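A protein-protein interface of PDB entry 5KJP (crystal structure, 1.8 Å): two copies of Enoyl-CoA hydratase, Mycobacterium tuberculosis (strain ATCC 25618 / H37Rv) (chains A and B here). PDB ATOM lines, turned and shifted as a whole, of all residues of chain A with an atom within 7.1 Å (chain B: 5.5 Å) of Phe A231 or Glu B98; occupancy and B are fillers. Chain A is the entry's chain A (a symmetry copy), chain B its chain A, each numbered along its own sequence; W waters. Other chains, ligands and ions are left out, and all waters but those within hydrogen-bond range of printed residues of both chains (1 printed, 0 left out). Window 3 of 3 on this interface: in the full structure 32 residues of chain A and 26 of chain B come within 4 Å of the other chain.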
ATOM      1  N   TRP A 225       3.306 -15.314   4.882  1.00  0.00           N
ATOM      2  CA  TRP A 225       3.867 -15.468   3.541  1.00  0.00           C
ATOM      3  C   TRP A 225       2.857 -16.102   2.594  1.00  0.00           C
ATOM      4  O   TRP A 225       2.041 -16.922   3.007  1.00  0.00           O
ATOM      5  CB  TRP A 225       5.137 -16.322   3.567  1.00  0.00           C
ATOM      6  CG  TRP A 225       6.250 -15.771   4.398  1.00  0.00           C
ATOM      7  CD1 TRP A 225       6.388 -14.492   4.847  1.00  0.00           C
ATOM      8  CD2 TRP A 225       7.393 -16.490   4.874  1.00  0.00           C
ATOM      9  NE1 TRP A 225       7.549 -14.368   5.578  1.00  0.00           N
ATOM     10  CE2 TRP A 225       8.182 -15.584   5.610  1.00  0.00           C
ATOM     11  CE3 TRP A 225       7.825 -17.817   4.749  1.00  0.00           C
ATOM     12  CZ2 TRP A 225       9.376 -15.961   6.221  1.00  0.00           C
ATOM     13  CZ3 TRP A 225       9.008 -18.189   5.357  1.00  0.00           C
ATOM     14  CH2 TRP A 225       9.770 -17.264   6.084  1.00  0.00           C
ATOM     15  N   SER A 226       2.918 -15.733   1.322  1.00  0.00           N
ATOM     16  CA  SER A 226       2.092 -16.382   0.311  1.00  0.00           C
ATOM     17  C   SER A 226       2.770 -17.668  -0.149  1.00  0.00           C
ATOM     18  O   SER A 226       3.997 -17.776  -0.084  1.00  0.00           O
ATOM     19  CB  SER A 226       1.855 -15.454  -0.878  1.00  0.00           C
ATOM     20  OG  SER A 226       3.044 -14.776  -1.238  1.00  0.00           O
ATOM     21  N   PRO A 227       1.975 -18.648  -0.606  1.00  0.00           N
ATOM     22  CA  PRO A 227       2.521 -19.880  -1.183  1.00  0.00           C
ATOM     23  C   PRO A 227       3.576 -19.605  -2.255  1.00  0.00           C
ATOM     24  O   PRO A 227       4.565 -20.328  -2.339  1.00  0.00           O
ATOM     25  CB  PRO A 227       1.290 -20.553  -1.791  1.00  0.00           C
ATOM     26  CG  PRO A 227       0.167 -20.096  -0.930  1.00  0.00           C
ATOM     27  CD  PRO A 227       0.502 -18.680  -0.543  1.00  0.00           C
ATOM     28  N   ASP A 228       3.368 -18.563  -3.051  1.00  0.00           N
ATOM     29  CA  ASP A 228       4.276 -18.254  -4.146  1.00  0.00           C
ATOM     30  C   ASP A 228       5.594 -17.648  -3.672  1.00  0.00           C
ATOM     31  O   ASP A 228       6.574 -17.648  -4.414  1.00  0.00           O
ATOM     32  CB  ASP A 228       3.603 -17.307  -5.143  1.00  0.00           C
ATOM     33  CG  ASP A 228       2.560 -18.006  -6.000  1.00  0.00           C
ATOM     34  OD1 ASP A 228       2.589 -19.253  -6.074  1.00  0.00           O
ATOM     35  OD2 ASP A 228       1.718 -17.308  -6.608  1.00  0.00           O
ATOM     36  N   THR A 229       5.629 -17.131  -2.448  1.00  0.00           N
ATOM     37  CA  THR A 229       6.844 -16.484  -1.962  1.00  0.00           C
ATOM     38  C   THR A 229       7.516 -17.218  -0.806  1.00  0.00           C
ATOM     39  O   THR A 229       8.642 -16.879  -0.440  1.00  0.00           O
ATOM     40  CB  THR A 229       6.574 -15.029  -1.502  1.00  0.00           C
ATOM     41  OG1 THR A 229       5.722 -15.028  -0.348  1.00  0.00           O
ATOM     42  CG2 THR A 229       5.928 -14.221  -2.622  1.00  0.00           C
ATOM     43  N   MET A 230       6.847 -18.223  -0.241  1.00  0.00           N
ATOM     44  CA  MET A 230       7.303 -18.803   1.024  1.00  0.00           C
ATOM     45  C   MET A 230       8.710 -19.411   0.947  1.00  0.00           C
ATOM     46  O   MET A 230       9.500 -19.255   1.876  1.00  0.00           O
ATOM     47  CB  MET A 230       6.288 -19.840   1.545  1.00  0.00           C
ATOM     48  CG  MET A 230       5.921 -20.995   0.614  1.00  0.00           C
ATOM     49  SD  MET A 230       4.568 -22.179   1.445  1.00  0.00           S
ATOM     50  CE  MET A 230       4.883 -23.795   0.393  1.00  0.00           C
ATOM     51  N   PHE A 231       9.044 -20.073  -0.153  1.00  0.00           N
ATOM     52  CA  PHE A 231      10.369 -20.676  -0.252  1.00  0.00           C
ATOM     53  C   PHE A 231      11.482 -19.630  -0.385  1.00  0.00           C
ATOM     54  O   PHE A 231      12.561 -19.793   0.190  1.00  0.00           O
ATOM     55  CB  PHE A 231      10.423 -21.670  -1.416  1.00  0.00           C
ATOM     56  CG  PHE A 231       9.997 -23.066  -1.035  1.00  0.00           C
ATOM     57  CD1 PHE A 231      10.869 -23.910  -0.361  1.00  0.00           C
ATOM     58  CD2 PHE A 231       8.723 -23.527  -1.337  1.00  0.00           C
ATOM     59  CE1 PHE A 231      10.482 -25.197  -0.002  1.00  0.00           C
ATOM     60  CE2 PHE A 231       8.329 -24.812  -0.983  1.00  0.00           C
ATOM     61  CZ  PHE A 231       9.209 -25.646  -0.311  1.00  0.00           C
ATOM     62  N   ALA A 232      11.220 -18.553  -1.125  1.00  0.00           N
ATOM     63  CA  ALA A 232      12.208 -17.479  -1.271  1.00  0.00           C
ATOM     64  C   ALA A 232      12.395 -16.709   0.044  1.00  0.00           C
ATOM     65  O   ALA A 232      13.516 -16.362   0.417  1.00  0.00           O
ATOM     66  CB  ALA A 232      11.803 -16.533  -2.396  1.00  0.00           C
ATOM     67  N   GLU A 233      11.296 -16.450   0.745  1.00  0.00           N
ATOM     68  CA  GLU A 233      11.358 -15.823   2.062  1.00  0.00           C
ATOM     69  C   GLU A 233      12.114 -16.702   3.057  1.00  0.00           C
ATOM     70  O   GLU A 233      12.911 -16.213   3.860  1.00  0.00           O
ATOM     71  CB  GLU A 233       9.948 -15.535   2.586  1.00  0.00           C
ATOM     72  CG  GLU A 233       9.152 -14.536   1.756  1.00  0.00           C
ATOM     73  CD  GLU A 233       9.591 -13.096   1.974  1.00  0.00           C
ATOM     74  OE1 GLU A 233      10.679 -12.870   2.545  1.00  0.00           O
ATOM     75  OE2 GLU A 233       8.835 -12.186   1.575  1.00  0.00           O
ATOM     76  N   GLN A 234      11.860 -18.004   2.988  1.00  0.00           N
ATOM     77  CA  GLN A 234      12.531 -18.965   3.852  1.00  0.00           C
ATOM     78  C   GLN A 234      14.043 -19.006   3.617  1.00  0.00           C
ATOM     79  O   GLN A 234      14.827 -19.085   4.565  1.00  0.00           O
ATOM     80  CB  GLN A 234      11.936 -20.363   3.647  1.00  0.00           C
ATOM     81  CG  GLN A 234      12.604 -21.431   4.488  1.00  0.00           C
ATOM     82  CD  GLN A 234      12.020 -22.808   4.250  1.00  0.00           C
ATOM     83  OE1 GLN A 234      11.354 -23.363   5.121  1.00  0.00           O
ATOM     84  NE2 GLN A 234      12.270 -23.367   3.068  1.00  0.00           N
ATOM     85  N   MET A 235      14.435 -18.950   2.345  1.00  0.00           N
ATOM     86  CA  MET A 235      15.837 -19.026   1.942  1.00  0.00           C
ATOM     87  C   MET A 235      16.706 -17.973   2.633  1.00  0.00           C
ATOM     88  O   MET A 235      17.843 -18.248   3.015  1.00  0.00           O
ATOM     89  CB  MET A 235      15.951 -18.875   0.419  1.00  0.00           C
ATOM     90  CG  MET A 235      17.358 -19.053  -0.130  1.00  0.00           C
ATOM     91  SD  MET A 235      18.146 -20.771   0.348  1.00  0.00           S
ATOM     92  CE  MET A 235      17.172 -21.906  -0.900  1.00  0.00           C
ATOM     93  N   LYS A 236      16.163 -16.769   2.790  1.00  0.00           N
ATOM     94  CA  LYS A 236      16.890 -15.668   3.424  1.00  0.00           C
ATOM     95  C   LYS A 236      17.251 -16.003   4.866  1.00  0.00           C
ATOM     96  O   LYS A 236      18.278 -15.568   5.386  1.00  0.00           O
ATOM     97  CB  LYS A 236      16.063 -14.385   3.391  1.00  0.00           C
ATOM     98  CG  LYS A 236      15.607 -13.959   2.004  1.00  0.00           C
ATOM     99  CD  LYS A 236      14.542 -12.875   2.111  1.00  0.00           C
ATOM    100  CE  LYS A 236      14.131 -12.352   0.745  1.00  0.00           C
ATOM    101  NZ  LYS A 236      12.859 -11.576   0.819  1.00  0.00           N
ATOM    102  N   LEU A 238      17.462 -19.242   5.879  1.00  0.00           N
ATOM    103  CA  LEU A 238      18.250 -20.476   5.813  1.00  0.00           C
ATOM    104  C   LEU A 238      19.748 -20.245   5.646  1.00  0.00           C
ATOM    105  O   LEU A 238      20.559 -20.928   6.273  1.00  0.00           O
ATOM    106  CB  LEU A 238      17.768 -21.364   4.660  1.00  0.00           C
ATOM    107  CG  LEU A 238      16.405 -22.046   4.772  1.00  0.00           C
ATOM    108  CD1 LEU A 238      16.160 -22.915   3.550  1.00  0.00           C
ATOM    109  CD2 LEU A 238      16.345 -22.880   6.033  1.00  0.00           C
ATOM    110  N   VAL B  88      19.346 -30.925  -4.720  1.00  0.00           N
ATOM    111  CA  VAL B  88      18.263 -29.953  -4.618  1.00  0.00           C
ATOM    112  C   VAL B  88      18.223 -29.132  -5.897  1.00  0.00           C
ATOM    113  O   VAL B  88      19.013 -28.206  -6.080  1.00  0.00           O
ATOM    114  CB  VAL B  88      18.420 -29.026  -3.401  1.00  0.00           C
ATOM    115  CG1 VAL B  88      17.233 -28.074  -3.307  1.00  0.00           C
ATOM    116  CG2 VAL B  88      18.544 -29.848  -2.121  1.00  0.00           C
ATOM    117  N   GLY B  91      13.977 -24.936  -9.015  1.00  0.00           N
ATOM    118  CA  GLY B  91      12.646 -25.018  -9.588  1.00  0.00           C
ATOM    119  C   GLY B  91      11.856 -26.246  -9.169  1.00  0.00           C
ATOM    120  O   GLY B  91      10.659 -26.333  -9.426  1.00  0.00           O
ATOM    121  N   ARG B  92      12.516 -27.199  -8.520  1.00  0.00           N
ATOM    122  CA  ARG B  92      11.858 -28.456  -8.166  1.00  0.00           C
ATOM    123  C   ARG B  92      12.105 -28.855  -6.718  1.00  0.00           C
ATOM    124  O   ARG B  92      11.270 -29.517  -6.104  1.00  0.00           O
ATOM    125  CB  ARG B  92      12.328 -29.585  -9.086  1.00  0.00           C
ATOM    126  CG  ARG B  92      11.949 -29.423 -10.552  1.00  0.00           C
ATOM    127  CD  ARG B  92      12.517 -30.573 -11.370  1.00  0.00           C
ATOM    128  NE  ARG B  92      12.210 -30.477 -12.798  1.00  0.00           N
ATOM    129  CZ  ARG B  92      11.061 -30.863 -13.349  1.00  0.00           C
ATOM    130  NH1 ARG B  92      10.088 -31.366 -12.599  1.00  0.00           N
ATOM    131  NH2 ARG B  92      10.885 -30.742 -14.660  1.00  0.00           N
ATOM    132  N   GLY B  93      13.261 -28.472  -6.186  1.00  0.00           N
ATOM    133  CA  GLY B  93      13.632 -28.819  -4.825  1.00  0.00           C
ATOM    134  C   GLY B  93      14.168 -30.236  -4.710  1.00  0.00           C
ATOM    135  O   GLY B  93      14.892 -30.718  -5.586  1.00  0.00           O
ATOM    136  N   LEU B  94      13.816 -30.904  -3.617  1.00  0.00           N
ATOM    137  CA  LEU B  94      14.221 -32.280  -3.405  1.00  0.00           C
ATOM    138  C   LEU B  94      13.268 -33.177  -4.173  1.00  0.00           C
ATOM    139  O   LEU B  94      12.230 -33.589  -3.655  1.00  0.00           O
ATOM    140  CB  LEU B  94      14.223 -32.628  -1.911  1.00  0.00           C
ATOM    141  CG  LEU B  94      14.948 -33.911  -1.498  1.00  0.00           C
ATOM    142  CD1 LEU B  94      16.454 -33.755  -1.680  1.00  0.00           C
ATOM    143  CD2 LEU B  94      14.599 -34.304  -0.059  1.00  0.00           C
ATOM    144  N   PHE B  96      10.644 -32.988  -5.897  1.00  0.00           N
ATOM    145  CA  PHE B  96       9.451 -32.240  -6.275  1.00  0.00           C
ATOM    146  C   PHE B  96       8.905 -31.380  -5.126  1.00  0.00           C
ATOM    147  O   PHE B  96       7.792 -30.868  -5.210  1.00  0.00           O
ATOM    148  CB  PHE B  96       8.359 -33.206  -6.759  1.00  0.00           C
ATOM    149  CG  PHE B  96       7.918 -34.196  -5.711  1.00  0.00           C
ATOM    150  CD1 PHE B  96       8.630 -35.373  -5.501  1.00  0.00           C
ATOM    151  CD2 PHE B  96       6.805 -33.941  -4.919  1.00  0.00           C
ATOM    152  CE1 PHE B  96       8.233 -36.279  -4.523  1.00  0.00           C
ATOM    153  CE2 PHE B  96       6.403 -34.840  -3.941  1.00  0.00           C
ATOM    154  CZ  PHE B  96       7.114 -36.011  -3.741  1.00  0.00           C
ATOM    155  N   THR B  97       9.681 -31.221  -4.056  1.00  0.00           N
ATOM    156  CA  THR B  97       9.206 -30.473  -2.889  1.00  0.00           C
ATOM    157  C   THR B  97       8.833 -29.023  -3.197  1.00  0.00           C
ATOM    158  O   THR B  97       7.980 -28.451  -2.524  1.00  0.00           O
ATOM    159  CB  THR B  97      10.253 -30.452  -1.761  1.00  0.00           C
ATOM    160  OG1 THR B  97      11.521 -30.053  -2.295  1.00  0.00           O
ATOM    161  CG2 THR B  97      10.373 -31.830  -1.109  1.00  0.00           C
ATOM    162  N   GLU B  98       9.473 -28.423  -4.197  1.00  0.00           N
ATOM    163  CA  GLU B  98       9.149 -27.046  -4.561  1.00  0.00           C
ATOM    164  C   GLU B  98       8.326 -26.987  -5.843  1.00  0.00           C
ATOM    165  O   GLU B  98       8.119 -25.917  -6.418  1.00  0.00           O
ATOM    166  CB  GLU B  98      10.424 -26.219  -4.698  1.00  0.00           C
ATOM    167  CG  GLU B  98      11.175 -26.116  -3.384  1.00  0.00           C
ATOM    168  CD  GLU B  98      12.418 -25.265  -3.470  1.00  0.00           C
ATOM    169  OE1 GLU B  98      12.419 -24.279  -4.236  1.00  0.00           O
ATOM    170  OE2 GLU B  98      13.393 -25.584  -2.758  1.00  0.00           O
ATOM    171  N   ARG B  99       7.850 -28.147  -6.278  1.00  0.00           N
ATOM    172  CA  ARG B  99       7.021 -28.231  -7.474  1.00  0.00           C
ATOM    173  C   ARG B  99       6.099 -29.449  -7.385  1.00  0.00           C
ATOM    174  O   ARG B  99       6.258 -30.409  -8.141  1.00  0.00           O
ATOM    175  CB  ARG B  99       7.903 -28.305  -8.726  1.00  0.00           C
ATOM    176  CG  ARG B  99       7.150 -28.249 -10.050  1.00  0.00           C
ATOM    177  CD  ARG B  99       8.053 -28.635 -11.209  1.00  0.00           C
ATOM    178  NE  ARG B  99       7.296 -28.840 -12.442  1.00  0.00           N
ATOM    179  CZ  ARG B  99       6.813 -27.858 -13.200  1.00  0.00           C
ATOM    180  NH1 ARG B  99       7.007 -26.590 -12.860  1.00  0.00           N
ATOM    181  NH2 ARG B  99       6.135 -28.148 -14.303  1.00  0.00           N
ATOM    182  N   PRO B 100       5.135 -29.419  -6.449  1.00  0.00           N
ATOM    183  CA  PRO B 100       4.228 -30.561  -6.279  1.00  0.00           C
ATOM    184  C   PRO B 100       3.407 -30.799  -7.545  1.00  0.00           C
ATOM    185  O   PRO B 100       3.101 -29.842  -8.258  1.00  0.00           O
ATOM    186  CB  PRO B 100       3.329 -30.136  -5.104  1.00  0.00           C
ATOM    187  CG  PRO B 100       4.007 -28.960  -4.479  1.00  0.00           C
ATOM    188  CD  PRO B 100       4.786 -28.298  -5.558  1.00  0.00           C
ATOM    189  N   GLY B 147      14.607 -27.160   5.359  1.00  0.00           N
ATOM    190  CA  GLY B 147      14.243 -26.180   4.342  1.00  0.00           C
ATOM    191  C   GLY B 147      13.567 -26.707   3.082  1.00  0.00           C
ATOM    192  O   GLY B 147      13.386 -25.964   2.109  1.00  0.00           O
ATOM    193  N   GLY B 148      13.184 -27.977   3.083  1.00  0.00           N
ATOM    194  CA  GLY B 148      12.567 -28.562   1.906  1.00  0.00           C
ATOM    195  C   GLY B 148      11.052 -28.554   2.000  1.00  0.00           C
ATOM    196  O   GLY B 148      10.379 -29.371   1.374  1.00  0.00           O
ATOM    197  N   GLY B 149      10.511 -27.639   2.797  1.00  0.00           N
ATOM    198  CA  GLY B 149       9.069 -27.517   2.932  1.00  0.00           C
ATOM    199  C   GLY B 149       8.535 -28.059   4.242  1.00  0.00           C
ATOM    200  O   GLY B 149       7.361 -27.870   4.564  1.00  0.00           O
ATOM    201  N   LEU B 152       7.334 -25.296   6.341  1.00  0.00           N
ATOM    202  CA  LEU B 152       6.256 -24.571   5.681  1.00  0.00           C
ATOM    203  C   LEU B 152       4.964 -25.378   5.636  1.00  0.00           C
ATOM    204  O   LEU B 152       3.876 -24.807   5.574  1.00  0.00           O
ATOM    205  CB  LEU B 152       6.666 -24.182   4.256  1.00  0.00           C
ATOM    206  CG  LEU B 152       7.923 -23.325   4.134  1.00  0.00           C
ATOM    207  CD1 LEU B 152       8.265 -23.081   2.666  1.00  0.00           C
ATOM    208  CD2 LEU B 152       7.764 -22.003   4.892  1.00  0.00           C
ATOM    209  N   ARG B 153       5.079 -26.700   5.671  1.00  0.00           N
ATOM    210  CA  ARG B 153       3.903 -27.548   5.500  1.00  0.00           C
ATOM    211  C   ARG B 153       3.458 -28.286   6.767  1.00  0.00           C
ATOM    212  O   ARG B 153       2.259 -28.436   6.992  1.00  0.00           O
ATOM    213  CB  ARG B 153       4.154 -28.558   4.378  1.00  0.00           C
ATOM    214  CG  ARG B 153       4.230 -27.895   3.007  1.00  0.00           C
ATOM    215  CD  ARG B 153       4.660 -28.857   1.902  1.00  0.00           C
ATOM    216  NE  ARG B 153       4.609 -28.178   0.607  1.00  0.00           N
ATOM    217  CZ  ARG B 153       5.575 -28.213  -0.305  1.00  0.00           C
ATOM    218  NH1 ARG B 153       6.684 -28.903  -0.078  1.00  0.00           N
ATOM    219  NH2 ARG B 153       5.428 -27.551  -1.449  1.00  0.00           N
HETATM  220  O   HOH W   1      10.784 -25.906   5.048  1.00  0.00           O
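The side-chain amide nitrogen (NE2) of Gln A234 is in hydrogen-bond range of the backbone carbonyl oxygen (O) of Gly B147, 3.0 Å away.
O of Arg B92 lies within hydrogen-bond range of N of Glu B98 (2.8 Å). The backbone NH (N) of Thr B97 is in hydrogen-bond range of the backbone carbonyl oxygen (O) of Arg B92 (3.1 Å). The backbone carbonyl oxygen (O) of Thr B97 sits at hydrogen-bond distance from the guanidinium group (NH1) of Arg B153 (2.8 Å). N of Leu B94 lies within hydrogen-bond range of OG1 of Thr B97.
Met A230 touches Leu B152 (CG to CD1, 3.7 Å). O of Thr B97 touches CZ of Phe A231, 3.8 Å away. Phe A231 touches Glu B98. CE1 of Phe A231 touches O of Gly B147, 3.7 Å away. Gly B148 touches Phe A231 (C to CE1, 3.9 Å). Gly B149 touches Phe A231. Leu B152 touches Gln A234. CA of Gly B147 touches CD1 of Leu A238, at 3.9 Å.
Of the printed residues of chain B, Phe A231 touches Thr B97, Glu B98, Gly B147, Gly B148 and Gly B149. Of chain A, only Phe A231 comes within 4 Å of Glu B98. Of the printed residues of chain A, Thr B97 touches Phe A231 (3.8 Å). Printed residues of chain B within 4 Å of Gln A234: Gly B147 and Leu B152. Of the printed residues of chain A, Gly B148 touches Phe A231. Of the printed residues of chain A, Gly B149 touches Phe A231 (3.7 Å). Thr A229 touches none of the printed residues of chain B. The nearest printed residue of chain B that does not touch Phe A231 is Arg B153 (4.02 Å).
Of the 13 printed residues of chain A, 4 touch a printed residue of chain B. Printed residues of chain A that touch a printed residue of chain B: Met A230, Phe A231, Gln A234 and Leu A238. Of the 15 printed residues of chain B, 6 touch a printed residue of chain A. Printed residues of chain B that touch a printed residue of chain A: Thr B97, Glu B98, Gly B147, Gly B148, Gly B149 and Leu B152. Hydrophobic or aromatic side chains of chain B within 4 Å of the printed part of chain A: Leu B152. Along chain B the printed residues that touch a printed residue of chain A span positions 97 to 152. Among the printed residues, 9 pairs touch across the chains.
No position is printed for both chains. Of the 9 pairs that touch across the chains among the printed residues, none has its exchanged pair printed and touching as well.
Water W1 bridges the side-chain amide oxygen (OE1) of Gln A234 and the backbone NH (N) of Gly B149.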
